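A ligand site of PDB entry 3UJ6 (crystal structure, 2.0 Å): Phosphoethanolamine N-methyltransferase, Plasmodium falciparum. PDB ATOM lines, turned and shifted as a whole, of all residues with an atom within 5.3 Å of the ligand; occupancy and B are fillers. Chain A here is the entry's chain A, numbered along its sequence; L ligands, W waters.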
ATOM      1  N   LEU A  14      31.957  25.283 -13.963  1.00  0.00           N
ATOM      2  CA  LEU A  14      31.866  23.854 -14.305  1.00  0.00           C
ATOM      3  C   LEU A  14      30.967  23.586 -15.518  1.00  0.00           C
ATOM      4  O   LEU A  14      31.348  22.822 -16.417  1.00  0.00           O
ATOM      5  CB  LEU A  14      31.392  23.019 -13.108  1.00  0.00           C
ATOM      6  CG  LEU A  14      32.349  22.968 -11.903  1.00  0.00           C
ATOM      7  CD1 LEU A  14      31.766  22.165 -10.752  1.00  0.00           C
ATOM      8  CD2 LEU A  14      33.695  22.408 -12.304  1.00  0.00           C
ATOM      9  N   TYR A  19      32.305  20.564 -17.868  1.00  0.00           N
ATOM     10  CA  TYR A  19      31.064  19.801 -17.976  1.00  0.00           C
ATOM     11  C   TYR A  19      29.974  20.409 -18.865  1.00  0.00           C
ATOM     12  O   TYR A  19      28.784  20.351 -18.530  1.00  0.00           O
ATOM     13  CB  TYR A  19      30.499  19.457 -16.588  1.00  0.00           C
ATOM     14  CG  TYR A  19      31.488  18.716 -15.696  1.00  0.00           C
ATOM     15  CD1 TYR A  19      31.918  17.428 -16.018  1.00  0.00           C
ATOM     16  CD2 TYR A  19      31.984  19.299 -14.545  1.00  0.00           C
ATOM     17  CE1 TYR A  19      32.823  16.746 -15.209  1.00  0.00           C
ATOM     18  CE2 TYR A  19      32.880  18.617 -13.725  1.00  0.00           C
ATOM     19  CZ  TYR A  19      33.303  17.348 -14.063  1.00  0.00           C
ATOM     20  OH  TYR A  19      34.191  16.687 -13.242  1.00  0.00           O
ATOM     21  N   ASN A  34      26.375   6.012 -18.567  1.00  0.00           N
ATOM     22  CA  ASN A  34      25.888   6.543 -17.284  1.00  0.00           C
ATOM     23  C   ASN A  34      26.998   6.948 -16.323  1.00  0.00           C
ATOM     24  O   ASN A  34      26.724   7.378 -15.196  1.00  0.00           O
ATOM     25  CB  ASN A  34      24.903   5.582 -16.609  1.00  0.00           C
ATOM     26  CG  ASN A  34      23.735   5.232 -17.500  1.00  0.00           C
ATOM     27  OD1 ASN A  34      23.225   6.078 -18.244  1.00  0.00           O
ATOM     28  ND2 ASN A  34      23.311   3.979 -17.439  1.00  0.00           N
ATOM     29  N   TYR A  35      28.240   6.807 -16.762  1.00  0.00           N
ATOM     30  CA  TYR A  35      29.392   7.146 -15.925  1.00  0.00           C
ATOM     31  C   TYR A  35      30.261   8.262 -16.518  1.00  0.00           C
ATOM     32  O   TYR A  35      30.459   8.330 -17.726  1.00  0.00           O
ATOM     33  CB  TYR A  35      30.250   5.902 -15.656  1.00  0.00           C
ATOM     34  CG  TYR A  35      29.550   4.911 -14.763  1.00  0.00           C
ATOM     35  CD1 TYR A  35      28.767   3.902 -15.289  1.00  0.00           C
ATOM     36  CD2 TYR A  35      29.631   5.030 -13.376  1.00  0.00           C
ATOM     37  CE1 TYR A  35      28.107   2.999 -14.468  1.00  0.00           C
ATOM     38  CE2 TYR A  35      28.985   4.132 -12.541  1.00  0.00           C
ATOM     39  CZ  TYR A  35      28.221   3.123 -13.088  1.00  0.00           C
ATOM     40  OH  TYR A  35      27.577   2.254 -12.251  1.00  0.00           O
ATOM     41  N   ILE A  36      30.758   9.131 -15.646  1.00  0.00           N
ATOM     42  CA  ILE A  36      31.769  10.103 -16.040  1.00  0.00           C
ATOM     43  C   ILE A  36      32.961  10.114 -15.072  1.00  0.00           C
ATOM     44  O   ILE A  36      33.531  11.155 -14.781  1.00  0.00           O
ATOM     45  CB  ILE A  36      31.188  11.531 -16.261  1.00  0.00           C
ATOM     46  CG1 ILE A  36      30.418  12.005 -15.035  1.00  0.00           C
ATOM     47  CG2 ILE A  36      30.261  11.548 -17.485  1.00  0.00           C
ATOM     48  CD1 ILE A  36      29.775  13.407 -15.227  1.00  0.00           C
ATOM     49  N   SER A  37      33.326   8.937 -14.581  1.00  0.00           N
ATOM     50  CA  SER A  37      34.505   8.817 -13.732  1.00  0.00           C
ATOM     51  C   SER A  37      35.155   7.444 -13.839  1.00  0.00           C
ATOM     52  O   SER A  37      34.577   6.490 -14.375  1.00  0.00           O
ATOM     53  CB  SER A  37      34.154   9.125 -12.275  1.00  0.00           C
ATOM     54  OG  SER A  37      33.595   7.980 -11.637  1.00  0.00           O
ATOM     55  N   ASP A  61      24.495  10.298  -2.756  1.00  0.00           N
ATOM     56  CA  ASP A  61      25.594  10.276  -3.710  1.00  0.00           C
ATOM     57  C   ASP A  61      25.995  11.721  -4.022  1.00  0.00           C
ATOM     58  O   ASP A  61      25.250  12.478  -4.639  1.00  0.00           O
ATOM     59  CB  ASP A  61      25.187   9.530  -4.999  1.00  0.00           C
ATOM     60  CG  ASP A  61      26.338   9.427  -6.009  1.00  0.00           C
ATOM     61  OD1 ASP A  61      27.373  10.111  -5.824  1.00  0.00           O
ATOM     62  OD2 ASP A  61      26.219   8.665  -6.999  1.00  0.00           O
ATOM     63  N   ILE A  62      27.187  12.098  -3.581  1.00  0.00           N
ATOM     64  CA  ILE A  62      27.651  13.472  -3.695  1.00  0.00           C
ATOM     65  C   ILE A  62      28.428  13.649  -4.993  1.00  0.00           C
ATOM     66  O   ILE A  62      29.492  13.060  -5.164  1.00  0.00           O
ATOM     67  CB  ILE A  62      28.523  13.871  -2.501  1.00  0.00           C
ATOM     68  CG1 ILE A  62      27.681  13.804  -1.219  1.00  0.00           C
ATOM     69  CG2 ILE A  62      29.110  15.266  -2.692  1.00  0.00           C
ATOM     70  CD1 ILE A  62      28.482  14.096   0.056  1.00  0.00           C
ATOM     71  N   GLY A  63      27.869  14.461  -5.882  1.00  0.00           N
ATOM     72  CA  GLY A  63      28.397  14.618  -7.225  1.00  0.00           C
ATOM     73  C   GLY A  63      27.925  13.469  -8.098  1.00  0.00           C
ATOM     74  O   GLY A  63      28.723  12.755  -8.692  1.00  0.00           O
ATOM     75  N   SER A  64      26.605  13.301  -8.183  1.00  0.00           N
ATOM     76  CA  SER A  64      26.012  12.082  -8.759  1.00  0.00           C
ATOM     77  C   SER A  64      26.166  11.921 -10.271  1.00  0.00           C
ATOM     78  O   SER A  64      25.949  10.837 -10.810  1.00  0.00           O
ATOM     79  CB  SER A  64      24.533  11.945  -8.349  1.00  0.00           C
ATOM     80  OG  SER A  64      23.843  13.173  -8.535  1.00  0.00           O
ATOM     81  N   GLY A  65      26.528  12.995 -10.961  1.00  0.00           N
ATOM     82  CA  GLY A  65      26.796  12.926 -12.385  1.00  0.00           C
ATOM     83  C   GLY A  65      25.625  12.434 -13.208  1.00  0.00           C
ATOM     84  O   GLY A  65      24.490  12.888 -13.034  1.00  0.00           O
ATOM     85  N   LEU A  66      25.877  11.493 -14.121  1.00  0.00           N
ATOM     86  CA  LEU A  66      24.828  10.991 -14.992  1.00  0.00           C
ATOM     87  C   LEU A  66      23.974   9.950 -14.277  1.00  0.00           C
ATOM     88  O   LEU A  66      23.013   9.428 -14.847  1.00  0.00           O
ATOM     89  CB  LEU A  66      25.419  10.380 -16.252  1.00  0.00           C
ATOM     90  CG  LEU A  66      26.084  11.403 -17.179  1.00  0.00           C
ATOM     91  CD1 LEU A  66      26.613  10.723 -18.439  1.00  0.00           C
ATOM     92  CD2 LEU A  66      25.068  12.477 -17.521  1.00  0.00           C
ATOM     93  N   ILE A  84      23.071  14.283  -5.557  1.00  0.00           N
ATOM     94  CA  ILE A  84      23.219  15.722  -5.663  1.00  0.00           C
ATOM     95  C   ILE A  84      24.349  16.055  -6.611  1.00  0.00           C
ATOM     96  O   ILE A  84      25.446  15.490  -6.514  1.00  0.00           O
ATOM     97  CB  ILE A  84      23.529  16.370  -4.299  1.00  0.00           C
ATOM     98  CG1 ILE A  84      22.444  16.056  -3.287  1.00  0.00           C
ATOM     99  CG2 ILE A  84      23.698  17.884  -4.453  1.00  0.00           C
ATOM    100  CD1 ILE A  84      21.231  16.935  -3.432  1.00  0.00           C
ATOM    101  N   ASP A  85      24.096  16.970  -7.540  1.00  0.00           N
ATOM    102  CA  ASP A  85      25.123  17.423  -8.452  1.00  0.00           C
ATOM    103  C   ASP A  85      24.898  18.896  -8.762  1.00  0.00           C
ATOM    104  O   ASP A  85      23.762  19.328  -8.994  1.00  0.00           O
ATOM    105  CB  ASP A  85      25.108  16.598  -9.735  1.00  0.00           C
ATOM    106  CG  ASP A  85      26.405  16.681 -10.487  1.00  0.00           C
ATOM    107  OD1 ASP A  85      26.642  17.725 -11.141  1.00  0.00           O
ATOM    108  OD2 ASP A  85      27.202  15.715 -10.399  1.00  0.00           O
ATOM    109  N   ILE A  86      25.968  19.681  -8.781  1.00  0.00           N
ATOM    110  CA  ILE A  86      25.831  21.128  -8.906  1.00  0.00           C
ATOM    111  C   ILE A  86      25.484  21.566 -10.343  1.00  0.00           C
ATOM    112  O   ILE A  86      24.918  22.637 -10.544  1.00  0.00           O
ATOM    113  CB  ILE A  86      27.111  21.836  -8.405  1.00  0.00           C
ATOM    114  CG1 ILE A  86      26.868  23.337  -8.201  1.00  0.00           C
ATOM    115  CG2 ILE A  86      28.280  21.600  -9.356  1.00  0.00           C
ATOM    116  CD1 ILE A  86      27.956  24.002  -7.353  1.00  0.00           C
ATOM    117  N   CYS A  87      25.808  20.741 -11.326  1.00  0.00           N
ATOM    118  CA  CYS A  87      25.568  21.094 -12.726  1.00  0.00           C
ATOM    119  C   CYS A  87      24.162  20.718 -13.168  1.00  0.00           C
ATOM    120  O   CYS A  87      23.835  19.545 -13.280  1.00  0.00           O
ATOM    121  CB  CYS A  87      26.613  20.444 -13.643  1.00  0.00           C
ATOM    122  SG  CYS A  87      28.304  21.086 -13.412  1.00  0.00           S
ATOM    123  N   ILE A  90      23.837  18.402 -16.264  1.00  0.00           N
ATOM    124  CA  ILE A  90      24.132  17.010 -15.937  1.00  0.00           C
ATOM    125  C   ILE A  90      22.926  16.331 -15.264  1.00  0.00           C
ATOM    126  O   ILE A  90      22.601  15.188 -15.581  1.00  0.00           O
ATOM    127  CB  ILE A  90      25.369  16.927 -15.012  1.00  0.00           C
ATOM    128  CG1 ILE A  90      26.628  17.319 -15.787  1.00  0.00           C
ATOM    129  CG2 ILE A  90      25.520  15.519 -14.470  1.00  0.00           C
ATOM    130  CD1 ILE A  90      27.909  17.286 -14.909  1.00  0.00           C
ATOM    131  N   ASN A 109      22.067  20.937  -7.145  1.00  0.00           N
ATOM    132  CA  ASN A 109      22.349  21.771  -5.979  1.00  0.00           C
ATOM    133  C   ASN A 109      23.828  21.662  -5.636  1.00  0.00           C
ATOM    134  O   ASN A 109      24.472  20.668  -5.943  1.00  0.00           O
ATOM    135  CB  ASN A 109      21.503  21.309  -4.792  1.00  0.00           C
ATOM    136  CG  ASN A 109      20.910  22.461  -4.016  1.00  0.00           C
ATOM    137  OD1 ASN A 109      21.573  23.070  -3.166  1.00  0.00           O
ATOM    138  ND2 ASN A 109      19.643  22.765  -4.274  1.00  0.00           N
ATOM    139  N   ASP A 110      24.375  22.714  -5.014  1.00  0.00           N
ATOM    140  CA  ASP A 110      25.717  22.679  -4.451  1.00  0.00           C
ATOM    141  C   ASP A 110      25.634  21.869  -3.150  1.00  0.00           C
ATOM    142  O   ASP A 110      24.835  22.187  -2.284  1.00  0.00           O
ATOM    143  CB  ASP A 110      26.158  24.111  -4.133  1.00  0.00           C
ATOM    144  CG  ASP A 110      27.597  24.219  -3.676  1.00  0.00           C
ATOM    145  OD1 ASP A 110      28.222  23.191  -3.330  1.00  0.00           O
ATOM    146  OD2 ASP A 110      28.098  25.365  -3.632  1.00  0.00           O
ATOM    147  N   ILE A 111      26.452  20.822  -3.011  1.00  0.00           N
ATOM    148  CA  ILE A 111      26.363  20.001  -1.803  1.00  0.00           C
ATOM    149  C   ILE A 111      26.690  20.834  -0.564  1.00  0.00           C
ATOM    150  O   ILE A 111      26.227  20.536   0.538  1.00  0.00           O
ATOM    151  CB  ILE A 111      27.281  18.737  -1.870  1.00  0.00           C
ATOM    152  CG1 ILE A 111      26.956  17.782  -0.712  1.00  0.00           C
ATOM    153  CG2 ILE A 111      28.760  19.113  -1.830  1.00  0.00           C
ATOM    154  CD1 ILE A 111      25.519  17.289  -0.709  1.00  0.00           C
ATOM    155  N   LEU A 112      27.474  21.898  -0.755  1.00  0.00           N
ATOM    156  CA  LEU A 112      27.897  22.754   0.361  1.00  0.00           C
ATOM    157  C   LEU A 112      26.766  23.575   0.966  1.00  0.00           C
ATOM    158  O   LEU A 112      26.874  24.047   2.097  1.00  0.00           O
ATOM    159  CB  LEU A 112      29.041  23.681  -0.081  1.00  0.00           C
ATOM    160  CG  LEU A 112      30.355  22.958  -0.421  1.00  0.00           C
ATOM    161  CD1 LEU A 112      31.330  23.908  -1.067  1.00  0.00           C
ATOM    162  CD2 LEU A 112      30.951  22.324   0.826  1.00  0.00           C
ATOM    163  N   ARG A 127      32.185   9.618  -5.721  1.00  0.00           N
ATOM    164  CA  ARG A 127      33.214   9.095  -6.606  1.00  0.00           C
ATOM    165  C   ARG A 127      33.797  10.243  -7.447  1.00  0.00           C
ATOM    166  O   ARG A 127      33.115  10.807  -8.314  1.00  0.00           O
ATOM    167  CB  ARG A 127      32.600   8.028  -7.539  1.00  0.00           C
ATOM    168  CG  ARG A 127      31.972   6.839  -6.800  1.00  0.00           C
ATOM    169  CD  ARG A 127      33.067   5.976  -6.168  1.00  0.00           C
ATOM    170  NE  ARG A 127      34.020   5.561  -7.189  1.00  0.00           N
ATOM    171  CZ  ARG A 127      33.786   4.601  -8.080  1.00  0.00           C
ATOM    172  NH1 ARG A 127      32.639   3.929  -8.049  1.00  0.00           N
ATOM    173  NH2 ARG A 127      34.703   4.309  -8.989  1.00  0.00           N
ATOM    174  N   ASP A 128      35.057  10.591  -7.156  1.00  0.00           N
ATOM    175  CA  ASP A 128      35.820  11.559  -7.958  1.00  0.00           C
ATOM    176  C   ASP A 128      35.091  12.889  -8.184  1.00  0.00           C
ATOM    177  O   ASP A 128      35.035  13.395  -9.310  1.00  0.00           O
ATOM    178  CB  ASP A 128      36.228  10.938  -9.306  1.00  0.00           C
ATOM    179  CG  ASP A 128      37.045   9.661  -9.145  1.00  0.00           C
ATOM    180  OD1 ASP A 128      37.473   9.372  -8.007  1.00  0.00           O
ATOM    181  OD2 ASP A 128      37.241   8.955 -10.155  1.00  0.00           O
ATOM    182  N   ALA A 129      34.575  13.475  -7.097  1.00  0.00           N
ATOM    183  CA  ALA A 129      33.852  14.736  -7.187  1.00  0.00           C
ATOM    184  C   ALA A 129      34.425  15.785  -6.234  1.00  0.00           C
ATOM    185  O   ALA A 129      34.403  16.984  -6.510  1.00  0.00           O
ATOM    186  CB  ALA A 129      32.382  14.518  -6.876  1.00  0.00           C
ATOM    187  N   HIS A 132      36.919  18.872  -6.710  1.00  0.00           N
ATOM    188  CA  HIS A 132      36.467  20.193  -7.130  1.00  0.00           C
ATOM    189  C   HIS A 132      36.396  21.191  -5.982  1.00  0.00           C
ATOM    190  O   HIS A 132      36.349  22.395  -6.204  1.00  0.00           O
ATOM    191  CB  HIS A 132      35.092  20.087  -7.801  1.00  0.00           C
ATOM    192  CG  HIS A 132      35.127  19.446  -9.156  1.00  0.00           C
ATOM    193  ND1 HIS A 132      35.725  20.053 -10.240  1.00  0.00           N
ATOM    194  CD2 HIS A 132      34.646  18.263  -9.594  1.00  0.00           C
ATOM    195  CE1 HIS A 132      35.596  19.263 -11.298  1.00  0.00           C
ATOM    196  NE2 HIS A 132      34.950  18.180 -10.933  1.00  0.00           N
ATOM    197  N   LEU A 133      36.379  20.701  -4.740  1.00  0.00           N
ATOM    198  CA  LEU A 133      36.223  21.592  -3.585  1.00  0.00           C
ATOM    199  C   LEU A 133      37.565  22.105  -3.051  1.00  0.00           C
ATOM    200  O   LEU A 133      38.540  21.370  -3.020  1.00  0.00           O
ATOM    201  CB  LEU A 133      35.462  20.901  -2.451  1.00  0.00           C
ATOM    202  CG  LEU A 133      33.935  20.814  -2.542  1.00  0.00           C
ATOM    203  CD1 LEU A 133      33.464  20.288  -3.886  1.00  0.00           C
ATOM    204  CD2 LEU A 133      33.381  19.967  -1.421  1.00  0.00           C
HETATM  205  N1  LIG L   1      30.174  10.445  -9.377  1.00  0.00           N
HETATM  206  C1  LIG L   1      30.131  10.719 -10.792  1.00  0.00           C
HETATM  207  C2  LIG L   1      30.506   9.474 -11.562  1.00  0.00           C
HETATM  208  O1  LIG L   1      31.268   8.659 -11.047  1.00  0.00           O
HETATM  209  O2  LIG L   1      30.098   9.269 -12.713  1.00  0.00           O
HETATM  210  C3  LIG L   1      31.240  11.722 -11.062  1.00  0.00           C
HETATM  211  C4  LIG L   1      30.841  12.953 -11.832  1.00  0.00           C
HETATM  212  S1  LIG L   1      32.341  13.882 -12.185  1.00  0.00           S
HETATM  213  C5  LIG L   1      33.634  12.687 -11.760  1.00  0.00           C
HETATM  214  C6  LIG L   1      32.370  15.011 -10.756  1.00  0.00           C
HETATM  215  C7  LIG L   1      30.984  15.591 -10.454  1.00  0.00           C
HETATM  216  O3  LIG L   1      30.975  16.328  -9.233  1.00  0.00           O
HETATM  217  C8  LIG L   1      30.493  16.541 -11.535  1.00  0.00           C
HETATM  218  O4  LIG L   1      29.268  16.065 -12.056  1.00  0.00           O
HETATM  219  C9  LIG L   1      30.255  17.870 -10.832  1.00  0.00           C
HETATM  220  O5  LIG L   1      29.103  18.508 -11.327  1.00  0.00           O
HETATM  221  C10 LIG L   1      30.106  17.447  -9.374  1.00  0.00           C
HETATM  222  N2  LIG L   1      30.395  18.545  -8.411  1.00  0.00           N
HETATM  223  C11 LIG L   1      31.492  19.370  -8.354  1.00  0.00           C
HETATM  224  N3  LIG L   1      31.331  20.218  -7.312  1.00  0.00           N
HETATM  225  C12 LIG L   1      30.147  19.954  -6.703  1.00  0.00           C
HETATM  226  C13 LIG L   1      29.492  20.518  -5.613  1.00  0.00           C
HETATM  227  N4  LIG L   1      30.021  21.534  -4.929  1.00  0.00           N
HETATM  228  N5  LIG L   1      28.267  20.008  -5.247  1.00  0.00           N
HETATM  229  C14 LIG L   1      27.699  18.963  -5.939  1.00  0.00           C
HETATM  230  N6  LIG L   1      28.352  18.411  -7.002  1.00  0.00           N
HETATM  231  C15 LIG L   1      29.558  18.900  -7.386  1.00  0.00           C
HETATM  232  O   HOH W   1      31.441   5.957 -10.522  1.00  0.00           O
HETATM  233  O   HOH W   2      32.485  22.745  -6.735  1.00  0.00           O
HETATM  234  O   HOH W   3      27.609   7.745 -11.261  1.00  0.00           O
HETATM  235  O   HOH W   4      27.803   9.310 -13.461  1.00  0.00           O
HETATM  236  O   HOH W   5      28.531   8.334  -8.495  1.00  0.00           O
HETATM  237  O   HOH W   6      29.767  10.762  -6.576  1.00  0.00           O
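An oxygen (O1) of the ligand is in hydrogen-bond range of the side-chain hydroxyl of Ser 37 (2.5 Å). The side-chain carboxylate of Asp 85 lies within hydrogen-bond range of an oxygen (O5) of the ligand (2.6 Å). The backbone carbonyl oxygen (O) of Gly 63 is in hydrogen-bond range of a nitrogen (N1) of the ligand. A nitrogen (N4) of the ligand sits at hydrogen-bond distance from the side-chain carboxylate of Asp 110, at 2.9 Å. N of Ile 111 is in hydrogen-bond range of N5 of the ligand. N of Ile 36 lies within hydrogen-bond range of O2 of the ligand, at 3.0 Å. The backbone carbonyl oxygen (O) of Arg 127 lies within hydrogen-bond range of a nitrogen (N1) of the ligand, 3.1 Å away. A nitrogen (N6) of the ligand is in hydrogen-bond range of the backbone NH (N) of Ile 86 (3.2 Å). The side-chain sulfur of Cys 87 is in hydrogen-bond range of an oxygen (O5) of the ligand (3.4 Å).
The side-chain carboxylate (OD1) of Asp 85 is in hydrogen-bond range of the backbone NH (N) of Cys 87, 3.1 Å away. N of Asn 109 lies within hydrogen-bond range of O of Asp 85, 3.0 Å away. The backbone NH (N) of Ser 64 sits at hydrogen-bond distance from the side-chain carboxylate (OD2) of Asp 85 (3.3 Å). N of Gly 63 lies within hydrogen-bond range of O of Ile 84. The side-chain carboxylate of Asp 110 is in hydrogen-bond range of the backbone NH of Leu 112 (3.0 Å). The backbone carbonyl oxygen (O) of Asn 109 sits close to the backbone NH (N) of Ile 86 (3.4 Å). NE2 of His 132 is in hydrogen-bond range of OH of Tyr 19 (2.9 Å). The backbone NH (N) of Tyr 19 is in hydrogen-bond range of the backbone carbonyl oxygen (O) of Leu 14 (2.8 Å).
The side-chain hydroxyl (OH) of Tyr 19 sits close to a sulfur (S1) of the ligand, at 3.5 Å. Merely in contact with the ligand: Leu 14, Tyr 35, Ile 90, Asn 109, Asp 128, Ala 129, His 132 and Leu 133. Within 4 Å of the ligand: Leu 14, Tyr 19, Tyr 35, Ile 36, Ser 37, Gly 63, Asp 85, Ile 86, Cys 87, Ile 90, Asn 109, Asp 110, Ile 111, Arg 127, Asp 128, Ala 129, His 132 and Leu 133. The nearest printed residue that does not touch the ligand is Gly 65 (4.01 Å).
Water W4 lies within hydrogen-bond range of O2 of the ligand (2.4 Å), O of Asn 34 (2.8 Å) and N of Leu 66 (3.0 Å). Water W1 lies within hydrogen-bond range of an oxygen (O1) of the ligand (2.8 Å), the side-chain hydroxyl of Ser 37 (3.2 Å) and the guanidinium group of Arg 127 (3.4 Å). Water W5 bridges the side-chain carboxylate of Asp 61 (2.8 Å) and a nitrogen (N1) of the ligand (2.8 Å).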
